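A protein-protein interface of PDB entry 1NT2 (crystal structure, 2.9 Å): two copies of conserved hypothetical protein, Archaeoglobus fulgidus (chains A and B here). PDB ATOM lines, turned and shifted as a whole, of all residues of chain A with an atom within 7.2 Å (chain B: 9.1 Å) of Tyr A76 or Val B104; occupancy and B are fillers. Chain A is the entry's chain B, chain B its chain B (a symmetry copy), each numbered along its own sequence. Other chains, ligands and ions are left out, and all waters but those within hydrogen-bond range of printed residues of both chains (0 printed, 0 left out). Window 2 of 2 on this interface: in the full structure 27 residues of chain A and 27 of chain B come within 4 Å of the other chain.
Of chain B, only Ile B101, Val B104, Lys B105, Ser B107 and Ile B109 come within 4 Å of Tyr A76.
Of chain A, only Tyr A76 comes within 4 Å of Val B104.
Ala A79 touches one residue of chain B.
Of the printed residues of chain A, Lys B105 touches Glu A73 (3.0 Å) and Tyr A76 (3.5 Å).
Printed residues of chain B within 4 Å of Glu A73: Lys B105.
The nearest residue of chain A that does not touch Val B104 is Arg A75 (4.1 Å).
The nearest printed residue of chain B that does not touch Glu A130 is Ser B107 (4.6 Å).
Among the printed residues, merely in contact across the chains: Tyr A76 with Ile B101 (3.9 Å), Tyr A76 with Val B104 (3.7 Å), Tyr A76 with Lys B105 (3.5 Å), Tyr A76 with Ile B109 (3.3 Å), Ala A79 with Ile B101 (3.6 Å), Leu A80 with Ile B101 (3.6 Å), Lys A82 with Lys B97 (3.0 Å) and Glu A130 with Ile B109 (3.2 Å).
The side-chain amino group (NZ) of Lys B105 lies within salt-bridge range of the side-chain carboxylate (OE1) of Glu A73, 3.0 Å away.
The side-chain hydroxyl (OH) of Tyr A76 lies within hydrogen-bond range of the side-chain hydroxyl (OG) of Ser B107, at 3.1 Å.
Hydrophobic or aromatic side chains of chain B within 4 Å of the printed part of chain A: Ile B101, Val B104 and Ile B109.
Printed residues of chain A that touch a printed residue of chain B: Glu A73, Tyr A76, Ala A79, Leu A80, Lys A82 and Glu A130.
Hydrophobic or aromatic side chains of chain A within 4 Å of the printed part of chain B: Tyr A76, Ala A79 and Leu A80.
Among the printed residues, Asp or Glu carboxylates within 4 Å of a Lys or Arg side-chain nitrogen of the other chain: Glu A73 with Lys B105 (3.0 Å).
OE1 of Glu A130 lies within hydrogen-bond range of OH of Tyr A76, at 2.7 Å.
OD1 of Asp B100 is in salt-bridge range of NZ of Lys B97 (3.2 Å).
O of Ser B107 sits at hydrogen-bond distance from OG1 of Thr B110.
No position is printed for both chains.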
ATOM      1  N   ARG A  71     -21.969 -22.608 -33.712  1.00  0.00           N
ATOM      2  CA  ARG A  71     -21.780 -22.248 -32.314  1.00  0.00           C
ATOM      3  C   ARG A  71     -22.361 -23.320 -31.392  1.00  0.00           C
ATOM      4  O   ARG A  71     -21.923 -23.469 -30.254  1.00  0.00           O
ATOM      5  CB  ARG A  71     -22.473 -20.912 -32.018  1.00  0.00           C
ATOM      6  CG  ARG A  71     -21.673 -19.665 -32.369  1.00  0.00           C
ATOM      7  CD  ARG A  71     -22.479 -18.393 -32.074  1.00  0.00           C
ATOM      8  NE  ARG A  71     -23.453 -18.083 -33.124  1.00  0.00           N
ATOM      9  CZ  ARG A  71     -24.316 -17.066 -33.084  1.00  0.00           C
ATOM     10  NH1 ARG A  71     -24.340 -16.252 -32.039  1.00  0.00           N
ATOM     11  NH2 ARG A  71     -25.150 -16.849 -34.097  1.00  0.00           N
ATOM     12  N   ARG A  72     -23.352 -24.053 -31.895  1.00  0.00           N
ATOM     13  CA  ARG A  72     -24.042 -25.115 -31.150  1.00  0.00           C
ATOM     14  C   ARG A  72     -24.486 -24.695 -29.747  1.00  0.00           C
ATOM     15  O   ARG A  72     -24.687 -25.530 -28.866  1.00  0.00           O
ATOM     16  CB  ARG A  72     -23.173 -26.378 -31.072  1.00  0.00           C
ATOM     17  CG  ARG A  72     -23.082 -27.154 -32.390  1.00  0.00           C
ATOM     18  CD  ARG A  72     -22.576 -28.597 -32.194  1.00  0.00           C
ATOM     19  NE  ARG A  72     -21.238 -28.685 -31.588  1.00  0.00           N
ATOM     20  CZ  ARG A  72     -20.605 -29.830 -31.327  1.00  0.00           C
ATOM     21  NH1 ARG A  72     -21.186 -30.988 -31.619  1.00  0.00           N
ATOM     22  NH2 ARG A  72     -19.395 -29.820 -30.772  1.00  0.00           N
ATOM     23  N   GLU A  73     -24.664 -23.395 -29.558  1.00  0.00           N
ATOM     24  CA  GLU A  73     -25.080 -22.856 -28.275  1.00  0.00           C
ATOM     25  C   GLU A  73     -26.357 -23.516 -27.756  1.00  0.00           C
ATOM     26  O   GLU A  73     -26.533 -23.685 -26.551  1.00  0.00           O
ATOM     27  CB  GLU A  73     -25.303 -21.350 -28.399  1.00  0.00           C
ATOM     28  CG  GLU A  73     -25.322 -20.613 -27.071  1.00  0.00           C
ATOM     29  CD  GLU A  73     -23.929 -20.412 -26.500  1.00  0.00           C
ATOM     30  OE1 GLU A  73     -23.170 -21.402 -26.389  1.00  0.00           O
ATOM     31  OE2 GLU A  73     -23.593 -19.259 -26.159  1.00  0.00           O
ATOM     32  N   ASP A  74     -27.251 -23.875 -28.669  1.00  0.00           N
ATOM     33  CA  ASP A  74     -28.503 -24.500 -28.282  1.00  0.00           C
ATOM     34  C   ASP A  74     -28.242 -25.806 -27.562  1.00  0.00           C
ATOM     35  O   ASP A  74     -29.003 -26.197 -26.679  1.00  0.00           O
ATOM     36  CB  ASP A  74     -29.398 -24.720 -29.509  1.00  0.00           C
ATOM     37  CG  ASP A  74     -28.706 -25.499 -30.619  1.00  0.00           C
ATOM     38  OD1 ASP A  74     -27.516 -25.230 -30.896  1.00  0.00           O
ATOM     39  OD2 ASP A  74     -29.365 -26.372 -31.235  1.00  0.00           O
ATOM     40  N   ARG A  75     -27.150 -26.471 -27.928  1.00  0.00           N
ATOM     41  CA  ARG A  75     -26.778 -27.744 -27.309  1.00  0.00           C
ATOM     42  C   ARG A  75     -26.418 -27.476 -25.862  1.00  0.00           C
ATOM     43  O   ARG A  75     -26.919 -28.135 -24.953  1.00  0.00           O
ATOM     44  CB  ARG A  75     -25.574 -28.345 -28.020  1.00  0.00           C
ATOM     45  CG  ARG A  75     -25.723 -28.403 -29.518  1.00  0.00           C
ATOM     46  CD  ARG A  75     -26.765 -29.419 -29.928  1.00  0.00           C
ATOM     47  NE  ARG A  75     -26.986 -29.397 -31.371  1.00  0.00           N
ATOM     48  CZ  ARG A  75     -27.577 -30.376 -32.046  1.00  0.00           C
ATOM     49  NH1 ARG A  75     -28.004 -31.461 -31.404  1.00  0.00           N
ATOM     50  NH2 ARG A  75     -27.739 -30.270 -33.361  1.00  0.00           N
ATOM     51  N   TYR A  76     -25.533 -26.504 -25.666  1.00  0.00           N
ATOM     52  CA  TYR A  76     -25.109 -26.107 -24.335  1.00  0.00           C
ATOM     53  C   TYR A  76     -26.357 -26.002 -23.475  1.00  0.00           C
ATOM     54  O   TYR A  76     -26.390 -26.488 -22.349  1.00  0.00           O
ATOM     55  CB  TYR A  76     -24.401 -24.750 -24.387  1.00  0.00           C
ATOM     56  CG  TYR A  76     -24.099 -24.134 -23.037  1.00  0.00           C
ATOM     57  CD1 TYR A  76     -23.009 -24.551 -22.275  1.00  0.00           C
ATOM     58  CD2 TYR A  76     -24.887 -23.101 -22.538  1.00  0.00           C
ATOM     59  CE1 TYR A  76     -22.709 -23.943 -21.051  1.00  0.00           C
ATOM     60  CE2 TYR A  76     -24.601 -22.490 -21.322  1.00  0.00           C
ATOM     61  CZ  TYR A  76     -23.513 -22.909 -20.587  1.00  0.00           C
ATOM     62  OH  TYR A  76     -23.225 -22.268 -19.405  1.00  0.00           O
ATOM     63  N   VAL A  77     -27.401 -25.391 -24.020  1.00  0.00           N
ATOM     64  CA  VAL A  77     -28.630 -25.227 -23.262  1.00  0.00           C
ATOM     65  C   VAL A  77     -29.341 -26.548 -22.922  1.00  0.00           C
ATOM     66  O   VAL A  77     -29.841 -26.720 -21.809  1.00  0.00           O
ATOM     67  CB  VAL A  77     -29.603 -24.279 -23.997  1.00  0.00           C
ATOM     68  CG1 VAL A  77     -30.833 -24.043 -23.149  1.00  0.00           C
ATOM     69  CG2 VAL A  77     -28.907 -22.953 -24.291  1.00  0.00           C
ATOM     70  N   VAL A  78     -29.382 -27.488 -23.861  1.00  0.00           N
ATOM     71  CA  VAL A  78     -30.048 -28.761 -23.585  1.00  0.00           C
ATOM     72  C   VAL A  78     -29.328 -29.463 -22.424  1.00  0.00           C
ATOM     73  O   VAL A  78     -29.950 -29.866 -21.428  1.00  0.00           O
ATOM     74  CB  VAL A  78     -30.036 -29.683 -24.820  1.00  0.00           C
ATOM     75  CG1 VAL A  78     -31.126 -30.705 -24.704  1.00  0.00           C
ATOM     76  CG2 VAL A  78     -30.219 -28.871 -26.062  1.00  0.00           C
ATOM     77  N   ALA A  79     -28.014 -29.599 -22.560  1.00  0.00           N
ATOM     78  CA  ALA A  79     -27.216 -30.232 -21.531  1.00  0.00           C
ATOM     79  C   ALA A  79     -27.517 -29.523 -20.218  1.00  0.00           C
ATOM     80  O   ALA A  79     -27.615 -30.142 -19.156  1.00  0.00           O
ATOM     81  CB  ALA A  79     -25.747 -30.100 -21.869  1.00  0.00           C
ATOM     82  N   LEU A  80     -27.680 -28.212 -20.308  1.00  0.00           N
ATOM     83  CA  LEU A  80     -27.947 -27.404 -19.141  1.00  0.00           C
ATOM     84  C   LEU A  80     -29.274 -27.763 -18.477  1.00  0.00           C
ATOM     85  O   LEU A  80     -29.355 -27.879 -17.255  1.00  0.00           O
ATOM     86  CB  LEU A  80     -27.938 -25.933 -19.544  1.00  0.00           C
ATOM     87  CG  LEU A  80     -27.124 -25.012 -18.642  1.00  0.00           C
ATOM     88  CD1 LEU A  80     -25.706 -25.531 -18.545  1.00  0.00           C
ATOM     89  CD2 LEU A  80     -27.155 -23.599 -19.192  1.00  0.00           C
ATOM     90  N   VAL A  81     -30.314 -27.935 -19.290  1.00  0.00           N
ATOM     91  CA  VAL A  81     -31.640 -28.270 -18.781  1.00  0.00           C
ATOM     92  C   VAL A  81     -31.666 -29.682 -18.239  1.00  0.00           C
ATOM     93  O   VAL A  81     -32.380 -29.977 -17.276  1.00  0.00           O
ATOM     94  CB  VAL A  81     -32.693 -28.193 -19.872  1.00  0.00           C
ATOM     95  CG1 VAL A  81     -34.029 -28.606 -19.325  1.00  0.00           C
ATOM     96  CG2 VAL A  81     -32.767 -26.808 -20.405  1.00  0.00           C
ATOM     97  N   LYS A  82     -30.895 -30.557 -18.880  1.00  0.00           N
ATOM     98  CA  LYS A  82     -30.828 -31.945 -18.470  1.00  0.00           C
ATOM     99  C   LYS A  82     -30.031 -32.086 -17.190  1.00  0.00           C
ATOM    100  O   LYS A  82     -30.169 -33.065 -16.468  1.00  0.00           O
ATOM    101  CB  LYS A  82     -30.208 -32.799 -19.577  1.00  0.00           C
ATOM    102  CG  LYS A  82     -31.177 -33.178 -20.691  1.00  0.00           C
ATOM    103  CD  LYS A  82     -30.570 -34.236 -21.599  1.00  0.00           C
ATOM    104  CE  LYS A  82     -31.603 -34.838 -22.537  1.00  0.00           C
ATOM    105  NZ  LYS A  82     -32.088 -33.863 -23.551  1.00  0.00           N
ATOM    106  N   GLU A 130     -28.377 -19.429 -15.654  1.00  0.00           N
ATOM    107  CA  GLU A 130     -27.668 -19.643 -16.903  1.00  0.00           C
ATOM    108  C   GLU A 130     -28.606 -19.875 -18.090  1.00  0.00           C
ATOM    109  O   GLU A 130     -28.487 -19.207 -19.123  1.00  0.00           O
ATOM    110  CB  GLU A 130     -26.720 -20.834 -16.762  1.00  0.00           C
ATOM    111  CG  GLU A 130     -25.245 -20.469 -16.791  1.00  0.00           C
ATOM    112  CD  GLU A 130     -24.751 -20.090 -18.172  1.00  0.00           C
ATOM    113  OE1 GLU A 130     -23.537 -19.841 -18.319  1.00  0.00           O
ATOM    114  OE2 GLU A 130     -25.571 -20.045 -19.111  1.00  0.00           O
ATOM    115  N   ILE A 131     -29.533 -20.818 -17.957  1.00  0.00           N
ATOM    116  CA  ILE A 131     -30.440 -21.095 -19.052  1.00  0.00           C
ATOM    117  C   ILE A 131     -31.154 -19.812 -19.429  1.00  0.00           C
ATOM    118  O   ILE A 131     -31.557 -19.629 -20.577  1.00  0.00           O
ATOM    119  CB  ILE A 131     -31.456 -22.197 -18.691  1.00  0.00           C
ATOM    120  CG1 ILE A 131     -32.283 -21.784 -17.474  1.00  0.00           C
ATOM    121  CG2 ILE A 131     -30.724 -23.495 -18.420  1.00  0.00           C
ATOM    122  CD1 ILE A 131     -33.484 -20.901 -17.777  1.00  0.00           C
ATOM    123  N   VAL A 134     -28.560 -17.388 -21.702  1.00  0.00           N
ATOM    124  CA  VAL A 134     -28.537 -17.824 -23.098  1.00  0.00           C
ATOM    125  C   VAL A 134     -29.911 -17.701 -23.761  1.00  0.00           C
ATOM    126  O   VAL A 134     -30.085 -16.947 -24.718  1.00  0.00           O
ATOM    127  CB  VAL A 134     -28.084 -19.280 -23.230  1.00  0.00           C
ATOM    128  CG1 VAL A 134     -26.613 -19.343 -23.399  1.00  0.00           C
ATOM    129  CG2 VAL A 134     -28.488 -20.052 -22.008  1.00  0.00           C
ATOM    130  N   LYS B  97     -23.747 -35.756 -16.076  1.00  0.00           N
ATOM    131  CA  LYS B  97     -24.419 -34.571 -16.569  1.00  0.00           C
ATOM    132  C   LYS B  97     -23.460 -33.426 -16.858  1.00  0.00           C
ATOM    133  O   LYS B  97     -23.761 -32.574 -17.687  1.00  0.00           O
ATOM    134  CB  LYS B  97     -25.485 -34.122 -15.565  1.00  0.00           C
ATOM    135  CG  LYS B  97     -26.733 -34.991 -15.566  1.00  0.00           C
ATOM    136  CD  LYS B  97     -27.656 -34.621 -16.717  1.00  0.00           C
ATOM    137  CE  LYS B  97     -28.327 -35.840 -17.355  1.00  0.00           C
ATOM    138  NZ  LYS B  97     -27.436 -36.549 -18.328  1.00  0.00           N
ATOM    139  N   LEU B  98     -22.310 -33.403 -16.182  1.00  0.00           N
ATOM    140  CA  LEU B  98     -21.320 -32.339 -16.380  1.00  0.00           C
ATOM    141  C   LEU B  98     -20.458 -32.605 -17.599  1.00  0.00           C
ATOM    142  O   LEU B  98     -20.134 -31.691 -18.350  1.00  0.00           O
ATOM    143  CB  LEU B  98     -20.414 -32.195 -15.146  1.00  0.00           C
ATOM    144  CG  LEU B  98     -19.251 -31.178 -15.071  1.00  0.00           C
ATOM    145  CD1 LEU B  98     -18.133 -31.565 -16.014  1.00  0.00           C
ATOM    146  CD2 LEU B  98     -19.753 -29.788 -15.384  1.00  0.00           C
ATOM    147  N   GLU B  99     -20.059 -33.855 -17.785  1.00  0.00           N
ATOM    148  CA  GLU B  99     -19.249 -34.184 -18.943  1.00  0.00           C
ATOM    149  C   GLU B  99     -20.162 -34.028 -20.148  1.00  0.00           C
ATOM    150  O   GLU B  99     -19.701 -34.029 -21.284  1.00  0.00           O
ATOM    151  CB  GLU B  99     -18.712 -35.618 -18.855  1.00  0.00           C
ATOM    152  CG  GLU B  99     -17.756 -35.886 -17.676  1.00  0.00           C
ATOM    153  CD  GLU B  99     -16.500 -34.999 -17.678  1.00  0.00           C
ATOM    154  OE1 GLU B  99     -15.824 -34.894 -18.730  1.00  0.00           O
ATOM    155  OE2 GLU B  99     -16.184 -34.416 -16.614  1.00  0.00           O
ATOM    156  N   ASP B 100     -21.462 -33.896 -19.883  1.00  0.00           N
ATOM    157  CA  ASP B 100     -22.462 -33.718 -20.934  1.00  0.00           C
ATOM    158  C   ASP B 100     -22.364 -32.281 -21.391  1.00  0.00           C
ATOM    159  O   ASP B 100     -22.260 -32.013 -22.581  1.00  0.00           O
ATOM    160  CB  ASP B 100     -23.877 -33.992 -20.412  1.00  0.00           C
ATOM    161  CG  ASP B 100     -24.504 -35.237 -21.033  1.00  0.00           C
ATOM    162  OD1 ASP B 100     -25.722 -35.468 -20.825  1.00  0.00           O
ATOM    163  OD2 ASP B 100     -23.775 -35.985 -21.726  1.00  0.00           O
ATOM    164  N   ILE B 101     -22.409 -31.360 -20.436  1.00  0.00           N
ATOM    165  CA  ILE B 101     -22.280 -29.946 -20.742  1.00  0.00           C
ATOM    166  C   ILE B 101     -20.885 -29.733 -21.348  1.00  0.00           C
ATOM    167  O   ILE B 101     -20.738 -29.198 -22.450  1.00  0.00           O
ATOM    168  CB  ILE B 101     -22.360 -29.088 -19.469  1.00  0.00           C
ATOM    169  CG1 ILE B 101     -23.688 -29.299 -18.764  1.00  0.00           C
ATOM    170  CG2 ILE B 101     -22.194 -27.629 -19.815  1.00  0.00           C
ATOM    171  CD1 ILE B 101     -23.834 -28.454 -17.528  1.00  0.00           C
ATOM    172  N   ARG B 102     -19.873 -30.179 -20.603  1.00  0.00           N
ATOM    173  CA  ARG B 102     -18.454 -30.064 -20.952  1.00  0.00           C
ATOM    174  C   ARG B 102     -18.039 -30.610 -22.327  1.00  0.00           C
ATOM    175  O   ARG B 102     -16.983 -30.235 -22.842  1.00  0.00           O
ATOM    176  CB  ARG B 102     -17.624 -30.751 -19.865  1.00  0.00           C
ATOM    177  CG  ARG B 102     -16.135 -30.499 -19.955  1.00  0.00           C
ATOM    178  CD  ARG B 102     -15.719 -29.289 -19.124  1.00  0.00           C
ATOM    179  NE  ARG B 102     -15.727 -29.563 -17.683  1.00  0.00           N
ATOM    180  CZ  ARG B 102     -14.924 -30.435 -17.074  1.00  0.00           C
ATOM    181  NH1 ARG B 102     -14.035 -31.130 -17.774  1.00  0.00           N
ATOM    182  NH2 ARG B 102     -15.014 -30.617 -15.763  1.00  0.00           N
ATOM    183  N   ALA B 103     -18.848 -31.496 -22.909  1.00  0.00           N
ATOM    184  CA  ALA B 103     -18.541 -32.077 -24.219  1.00  0.00           C
ATOM    185  C   ALA B 103     -18.834 -31.027 -25.270  1.00  0.00           C
ATOM    186  O   ALA B 103     -18.343 -31.093 -26.405  1.00  0.00           O
ATOM    187  CB  ALA B 103     -19.392 -33.318 -24.466  1.00  0.00           C
ATOM    188  N   VAL B 104     -19.644 -30.055 -24.863  1.00  0.00           N
ATOM    189  CA  VAL B 104     -20.048 -28.940 -25.709  1.00  0.00           C
ATOM    190  C   VAL B 104     -19.195 -27.705 -25.363  1.00  0.00           C
ATOM    191  O   VAL B 104     -18.185 -27.431 -26.010  1.00  0.00           O
ATOM    192  CB  VAL B 104     -21.566 -28.644 -25.501  1.00  0.00           C
ATOM    193  CG1 VAL B 104     -21.991 -27.432 -26.286  1.00  0.00           C
ATOM    194  CG2 VAL B 104     -22.389 -29.849 -25.926  1.00  0.00           C
ATOM    195  N   LYS B 105     -19.584 -26.983 -24.320  1.00  0.00           N
ATOM    196  CA  LYS B 105     -18.867 -25.787 -23.910  1.00  0.00           C
ATOM    197  C   LYS B 105     -18.218 -25.951 -22.549  1.00  0.00           C
ATOM    198  O   LYS B 105     -18.724 -26.683 -21.703  1.00  0.00           O
ATOM    199  CB  LYS B 105     -19.830 -24.601 -23.858  1.00  0.00           C
ATOM    200  CG  LYS B 105     -19.219 -23.330 -23.310  1.00  0.00           C
ATOM    201  CD  LYS B 105     -20.280 -22.265 -23.013  1.00  0.00           C
ATOM    202  CE  LYS B 105     -20.900 -21.653 -24.270  1.00  0.00           C
ATOM    203  NZ  LYS B 105     -21.728 -20.440 -23.962  1.00  0.00           N
ATOM    204  N   GLU B 106     -17.096 -25.265 -22.345  1.00  0.00           N
ATOM    205  CA  GLU B 106     -16.380 -25.297 -21.067  1.00  0.00           C
ATOM    206  C   GLU B 106     -16.641 -23.936 -20.420  1.00  0.00           C
ATOM    207  O   GLU B 106     -15.738 -23.118 -20.264  1.00  0.00           O
ATOM    208  CB  GLU B 106     -14.876 -25.506 -21.305  1.00  0.00           C
ATOM    209  CG  GLU B 106     -13.969 -25.164 -20.115  1.00  0.00           C
ATOM    210  CD  GLU B 106     -13.994 -26.199 -19.008  1.00  0.00           C
ATOM    211  OE1 GLU B 106     -13.129 -27.105 -19.026  1.00  0.00           O
ATOM    212  OE2 GLU B 106     -14.876 -26.110 -18.124  1.00  0.00           O
ATOM    213  N   SER B 107     -17.892 -23.698 -20.051  1.00  0.00           N
ATOM    214  CA  SER B 107     -18.288 -22.430 -19.455  1.00  0.00           C
ATOM    215  C   SER B 107     -17.781 -22.194 -18.053  1.00  0.00           C
ATOM    216  O   SER B 107     -17.276 -23.089 -17.391  1.00  0.00           O
ATOM    217  CB  SER B 107     -19.807 -22.313 -19.449  1.00  0.00           C
ATOM    218  OG  SER B 107     -20.393 -23.437 -18.816  1.00  0.00           O
ATOM    219  N   GLU B 108     -17.937 -20.957 -17.609  1.00  0.00           N
ATOM    220  CA  GLU B 108     -17.515 -20.556 -16.283  1.00  0.00           C
ATOM    221  C   GLU B 108     -18.538 -21.010 -15.246  1.00  0.00           C
ATOM    222  O   GLU B 108     -18.565 -20.499 -14.122  1.00  0.00           O
ATOM    223  CB  GLU B 108     -17.338 -19.036 -16.230  1.00  0.00           C
ATOM    224  CG  GLU B 108     -16.196 -18.518 -17.115  1.00  0.00           C
ATOM    225  CD  GLU B 108     -16.062 -16.994 -17.108  1.00  0.00           C
ATOM    226  OE1 GLU B 108     -15.031 -16.481 -17.614  1.00  0.00           O
ATOM    227  OE2 GLU B 108     -16.988 -16.313 -16.608  1.00  0.00           O
ATOM    228  N   ILE B 109     -19.391 -21.958 -15.633  1.00  0.00           N
ATOM    229  CA  ILE B 109     -20.393 -22.506 -14.721  1.00  0.00           C
ATOM    230  C   ILE B 109     -20.111 -23.987 -14.562  1.00  0.00           C
ATOM    231  O   ILE B 109     -20.467 -24.585 -13.554  1.00  0.00           O
ATOM    232  CB  ILE B 109     -21.846 -22.327 -15.235  1.00  0.00           C
ATOM    233  CG1 ILE B 109     -22.833 -22.678 -14.116  1.00  0.00           C
ATOM    234  CG2 ILE B 109     -22.096 -23.233 -16.424  1.00  0.00           C
ATOM    235  CD1 ILE B 109     -24.215 -22.097 -14.292  1.00  0.00           C
ATOM    236  N   THR B 110     -19.476 -24.577 -15.571  1.00  0.00           N
ATOM    237  CA  THR B 110     -19.123 -25.987 -15.510  1.00  0.00           C
ATOM    238  C   THR B 110     -18.109 -26.109 -14.380  1.00  0.00           C
ATOM    239  O   THR B 110     -17.921 -27.181 -13.804  1.00  0.00           O
ATOM    240  CB  THR B 110     -18.474 -26.474 -16.823  1.00  0.00           C
ATOM    241  OG1 THR B 110     -17.335 -25.664 -17.124  1.00  0.00           O
ATOM    242  CG2 THR B 110     -19.455 -26.393 -17.971  1.00  0.00           C
ATOM    243  N   GLU B 111     -17.463 -24.991 -14.067  1.00  0.00           N
ATOM    244  CA  GLU B 111     -16.473 -24.962 -13.003  1.00  0.00           C
ATOM    245  C   GLU B 111     -17.154 -25.000 -11.653  1.00  0.00           C
ATOM    246  O   GLU B 111     -16.744 -25.760 -10.773  1.00  0.00           O
ATOM    247  CB  GLU B 111     -15.603 -23.708 -13.109  1.00  0.00           C
ATOM    248  CG  GLU B 111     -14.660 -23.715 -14.303  1.00  0.00           C
ATOM    249  CD  GLU B 111     -13.835 -24.997 -14.399  1.00  0.00           C
ATOM    250  OE1 GLU B 111     -13.114 -25.331 -13.426  1.00  0.00           O
ATOM    251  OE2 GLU B 111     -13.916 -25.672 -15.455  1.00  0.00           O
